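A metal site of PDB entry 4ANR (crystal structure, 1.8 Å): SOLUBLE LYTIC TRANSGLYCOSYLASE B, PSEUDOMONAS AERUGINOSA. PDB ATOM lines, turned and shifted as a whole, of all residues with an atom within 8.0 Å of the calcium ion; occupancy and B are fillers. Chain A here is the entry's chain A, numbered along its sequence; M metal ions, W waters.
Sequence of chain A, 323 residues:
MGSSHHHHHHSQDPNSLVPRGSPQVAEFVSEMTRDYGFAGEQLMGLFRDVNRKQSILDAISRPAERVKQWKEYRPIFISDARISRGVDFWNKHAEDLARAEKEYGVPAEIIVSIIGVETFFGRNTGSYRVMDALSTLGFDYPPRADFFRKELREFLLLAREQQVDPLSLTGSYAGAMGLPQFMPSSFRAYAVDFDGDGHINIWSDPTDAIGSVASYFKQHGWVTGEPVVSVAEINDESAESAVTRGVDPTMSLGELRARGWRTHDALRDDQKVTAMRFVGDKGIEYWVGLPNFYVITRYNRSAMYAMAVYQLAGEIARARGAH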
ATOM      1  N   GLN A 162      23.359 -20.013 -33.721  1.00  0.00           N
ATOM      2  CA  GLN A 162      24.317 -19.372 -32.807  1.00  0.00           C
ATOM      3  C   GLN A 162      25.627 -19.066 -33.547  1.00  0.00           C
ATOM      4  O   GLN A 162      26.525 -18.443 -32.993  1.00  0.00           O
ATOM      5  CB  GLN A 162      24.591 -20.265 -31.604  1.00  0.00           C
ATOM      6  CG  GLN A 162      23.357 -20.374 -30.688  1.00  0.00           C
ATOM      7  CD  GLN A 162      22.899 -19.007 -30.211  1.00  0.00           C
ATOM      8  OE1 GLN A 162      21.717 -18.656 -30.300  1.00  0.00           O
ATOM      9  NE2 GLN A 162      23.837 -18.220 -29.701  1.00  0.00           N
ATOM     10  N   VAL A 192      17.796 -18.591 -23.244  1.00  0.00           N
ATOM     11  CA  VAL A 192      17.745 -17.137 -23.479  1.00  0.00           C
ATOM     12  C   VAL A 192      19.112 -16.497 -23.346  1.00  0.00           C
ATOM     13  O   VAL A 192      20.015 -16.997 -22.646  1.00  0.00           O
ATOM     14  CB  VAL A 192      16.791 -16.407 -22.542  1.00  0.00           C
ATOM     15  CG1 VAL A 192      15.327 -16.854 -22.780  1.00  0.00           C
ATOM     16  CG2 VAL A 192      17.199 -16.570 -21.088  1.00  0.00           C
ATOM     17  N   ASP A 193      19.276 -15.386 -24.066  1.00  0.00           N
ATOM     18  CA  ASP A 193      20.485 -14.575 -23.985  1.00  0.00           C
ATOM     19  C   ASP A 193      20.177 -13.574 -22.894  1.00  0.00           C
ATOM     20  O   ASP A 193      19.440 -12.620 -23.130  1.00  0.00           O
ATOM     21  CB  ASP A 193      20.711 -13.838 -25.316  1.00  0.00           C
ATOM     22  CG  ASP A 193      21.799 -12.767 -25.229  1.00  0.00           C
ATOM     23  OD1 ASP A 193      22.586 -12.791 -24.248  1.00  0.00           O
ATOM     24  OD2 ASP A 193      21.891 -11.938 -26.164  1.00  0.00           O
ATOM     25  N   PHE A 194      20.676 -13.832 -21.685  1.00  0.00           N
ATOM     26  CA  PHE A 194      20.226 -13.080 -20.526  1.00  0.00           C
ATOM     27  C   PHE A 194      21.188 -11.937 -20.208  1.00  0.00           C
ATOM     28  O   PHE A 194      20.897 -11.124 -19.334  1.00  0.00           O
ATOM     29  CB  PHE A 194      20.090 -14.013 -19.304  1.00  0.00           C
ATOM     30  CG  PHE A 194      19.190 -13.465 -18.207  1.00  0.00           C
ATOM     31  CD1 PHE A 194      17.918 -12.971 -18.484  1.00  0.00           C
ATOM     32  CD2 PHE A 194      19.624 -13.483 -16.882  1.00  0.00           C
ATOM     33  CE1 PHE A 194      17.067 -12.513 -17.474  1.00  0.00           C
ATOM     34  CE2 PHE A 194      18.792 -12.991 -15.838  1.00  0.00           C
ATOM     35  CZ  PHE A 194      17.504 -12.516 -16.136  1.00  0.00           C
ATOM     36  N   ASP A 195      22.307 -11.856 -20.901  1.00  0.00           N
ATOM     37  CA  ASP A 195      23.149 -10.658 -20.738  1.00  0.00           C
ATOM     38  C   ASP A 195      23.246  -9.801 -21.989  1.00  0.00           C
ATOM     39  O   ASP A 195      24.110  -8.920 -22.077  1.00  0.00           O
ATOM     40  CB  ASP A 195      24.551 -10.993 -20.188  1.00  0.00           C
ATOM     41  CG  ASP A 195      25.251 -12.080 -20.989  1.00  0.00           C
ATOM     42  OD1 ASP A 195      24.858 -12.357 -22.142  1.00  0.00           O
ATOM     43  OD2 ASP A 195      26.209 -12.669 -20.441  1.00  0.00           O
ATOM     44  N   GLY A 196      22.381 -10.075 -22.962  1.00  0.00           N
ATOM     45  CA  GLY A 196      22.107  -9.123 -24.033  1.00  0.00           C
ATOM     46  C   GLY A 196      23.278  -8.913 -24.980  1.00  0.00           C
ATOM     47  O   GLY A 196      23.335  -7.887 -25.660  1.00  0.00           O
ATOM     48  N   ASP A 197      24.185  -9.883 -25.048  1.00  0.00           N
ATOM     49  CA  ASP A 197      25.331  -9.841 -25.949  1.00  0.00           C
ATOM     50  C   ASP A 197      25.115 -10.497 -27.320  1.00  0.00           C
ATOM     51  O   ASP A 197      26.032 -10.542 -28.128  1.00  0.00           O
ATOM     52  CB  ASP A 197      26.590 -10.416 -25.278  1.00  0.00           C
ATOM     53  CG  ASP A 197      26.560 -11.943 -25.162  1.00  0.00           C
ATOM     54  OD1 ASP A 197      25.469 -12.540 -25.358  1.00  0.00           O
ATOM     55  OD2 ASP A 197      27.616 -12.544 -24.896  1.00  0.00           O
ATOM     56  N   GLY A 198      23.910 -10.993 -27.586  1.00  0.00           N
ATOM     57  CA  GLY A 198      23.587 -11.611 -28.877  1.00  0.00           C
ATOM     58  C   GLY A 198      23.992 -13.077 -29.057  1.00  0.00           C
ATOM     59  O   GLY A 198      23.920 -13.622 -30.177  1.00  0.00           O
ATOM     60  N   HIS A 199      24.452 -13.704 -27.965  1.00  0.00           N
ATOM     61  CA  HIS A 199      24.833 -15.125 -27.978  1.00  0.00           C
ATOM     62  C   HIS A 199      24.054 -15.816 -26.863  1.00  0.00           C
ATOM     63  O   HIS A 199      23.760 -15.199 -25.834  1.00  0.00           O
ATOM     64  CB  HIS A 199      26.340 -15.288 -27.694  1.00  0.00           C
ATOM     65  CG  HIS A 199      27.226 -14.531 -28.637  1.00  0.00           C
ATOM     66  ND1 HIS A 199      27.351 -14.857 -29.969  1.00  0.00           N
ATOM     67  CD2 HIS A 199      28.026 -13.461 -28.441  1.00  0.00           C
ATOM     68  CE1 HIS A 199      28.189 -14.016 -30.553  1.00  0.00           C
ATOM     69  NE2 HIS A 199      28.614 -13.155 -29.645  1.00  0.00           N
ATOM     70  N   ILE A 200      23.712 -17.089 -27.062  1.00  0.00           N
ATOM     71  CA  ILE A 200      23.185 -17.898 -25.957  1.00  0.00           C
ATOM     72  C   ILE A 200      24.225 -18.956 -25.614  1.00  0.00           C
ATOM     73  O   ILE A 200      24.453 -19.895 -26.377  1.00  0.00           O
ATOM     74  CB  ILE A 200      21.830 -18.566 -26.325  1.00  0.00           C
ATOM     75  CG1 ILE A 200      20.761 -17.486 -26.596  1.00  0.00           C
ATOM     76  CG2 ILE A 200      21.360 -19.513 -25.174  1.00  0.00           C
ATOM     77  CD1 ILE A 200      19.359 -18.019 -26.943  1.00  0.00           C
ATOM     78  N   ASN A 201      24.933 -18.737 -24.520  1.00  0.00           N
ATOM     79  CA  ASN A 201      26.035 -19.596 -24.127  1.00  0.00           C
ATOM     80  C   ASN A 201      25.738 -20.175 -22.739  1.00  0.00           C
ATOM     81  O   ASN A 201      26.080 -19.584 -21.717  1.00  0.00           O
ATOM     82  CB  ASN A 201      27.349 -18.824 -24.110  1.00  0.00           C
ATOM     83  CG  ASN A 201      28.479 -19.616 -23.521  1.00  0.00           C
ATOM     84  OD1 ASN A 201      28.336 -20.806 -23.241  1.00  0.00           O
ATOM     85  ND2 ASN A 201      29.609 -18.957 -23.279  1.00  0.00           N
ATOM     86  N   ILE A 202      25.101 -21.348 -22.713  1.00  0.00           N
ATOM     87  CA  ILE A 202      24.836 -22.030 -21.458  1.00  0.00           C
ATOM     88  C   ILE A 202      26.016 -22.875 -20.937  1.00  0.00           C
ATOM     89  O   ILE A 202      25.904 -23.489 -19.880  1.00  0.00           O
ATOM     90  CB  ILE A 202      23.494 -22.867 -21.501  1.00  0.00           C
ATOM     91  CG1 ILE A 202      23.584 -23.997 -22.545  1.00  0.00           C
ATOM     92  CG2 ILE A 202      22.310 -21.963 -21.826  1.00  0.00           C
ATOM     93  CD1 ILE A 202      22.434 -25.061 -22.443  1.00  0.00           C
ATOM     94  N   ASP A 205      28.749 -19.282 -19.781  1.00  0.00           N
ATOM     95  CA  ASP A 205      28.231 -17.989 -19.377  1.00  0.00           C
ATOM     96  C   ASP A 205      27.147 -18.205 -18.343  1.00  0.00           C
ATOM     97  O   ASP A 205      26.009 -18.488 -18.687  1.00  0.00           O
ATOM     98  CB  ASP A 205      27.665 -17.231 -20.578  1.00  0.00           C
ATOM     99  CG  ASP A 205      27.173 -15.844 -20.212  1.00  0.00           C
ATOM    100  OD1 ASP A 205      27.060 -15.544 -18.990  1.00  0.00           O
ATOM    101  OD2 ASP A 205      26.925 -15.052 -21.143  1.00  0.00           O
ATOM    102  N   THR A 207      25.442 -16.291 -16.587  1.00  0.00           N
ATOM    103  CA  THR A 207      24.302 -15.390 -16.744  1.00  0.00           C
ATOM    104  C   THR A 207      23.227 -15.959 -17.677  1.00  0.00           C
ATOM    105  O   THR A 207      22.031 -15.916 -17.353  1.00  0.00           O
ATOM    106  CB  THR A 207      24.724 -13.983 -17.231  1.00  0.00           C
ATOM    107  OG1 THR A 207      25.680 -13.430 -16.321  1.00  0.00           O
ATOM    108  CG2 THR A 207      23.497 -13.052 -17.315  1.00  0.00           C
ATOM    109  N   ASP A 208      23.632 -16.431 -18.850  1.00  0.00           N
ATOM    110  CA  ASP A 208      22.682 -17.063 -19.791  1.00  0.00           C
ATOM    111  C   ASP A 208      22.099 -18.349 -19.171  1.00  0.00           C
ATOM    112  O   ASP A 208      20.920 -18.641 -19.341  1.00  0.00           O
ATOM    113  CB  ASP A 208      23.378 -17.453 -21.121  1.00  0.00           C
ATOM    114  CG  ASP A 208      23.687 -16.247 -22.039  1.00  0.00           C
ATOM    115  OD1 ASP A 208      23.151 -15.121 -21.840  1.00  0.00           O
ATOM    116  OD2 ASP A 208      24.522 -16.438 -22.957  1.00  0.00           O
ATOM    117  N   ALA A 209      22.936 -19.158 -18.515  1.00  0.00           N
ATOM    118  CA  ALA A 209      22.417 -20.370 -17.839  1.00  0.00           C
ATOM    119  C   ALA A 209      21.319 -20.041 -16.824  1.00  0.00           C
ATOM    120  O   ALA A 209      20.310 -20.733 -16.749  1.00  0.00           O
ATOM    121  CB  ALA A 209      23.544 -21.169 -17.161  1.00  0.00           C
HETATM  122 CA    CA M   1      24.453 -14.116 -23.828  1.00  0.00          CA
HETATM  123  O   HOH W   1      26.590 -14.769 -23.920  1.00  0.00           O
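Water W1 bridges OD2 of Asp 197 (2.6 Å) and OD2 of Asp 205 (2.8 Å).
Residues that only touch the calcium ion: Asp 205. Of the 16 residues printed, 6 come within 4 Å of the calcium ion. Along chain A the residues within 4 Å of the calcium ion span positions 193 to 208.
The calcium ion is bound by water W1 (2.2 Å), OD1 of Asp 193 (2.3 Å), O of His 199 (2.4 Å), OD1 of Asp 197 (2.4 Å), OD1 of Asp 195 (2.5 Å), OD2 of Asp 208 (2.5 Å) and OD1 of Asp 208 (2.6 Å). The calcium ion has seven donor atoms within binding distance.
The backbone NH of Gly 196 sits close to the side-chain carboxylate of Asp 193. OD2 of Asp 193 sits at hydrogen-bond distance from N of Gly 198, 2.6 Å away. The side-chain carboxylate (OD2) of Asp 195 sits close to the side-chain carboxylate (OD2) of Asp 205, 2.6 Å away. The side-chain carboxylate of Asp 208 sits close to the backbone NH of Phe 194, 2.8 Å away. N of Asn 201 lies close to OD2 of Asp 208. The side-chain carboxylate of Asp 205 lies within hydrogen-bond range of the backbone NH of Thr 207, 3.0 Å away.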
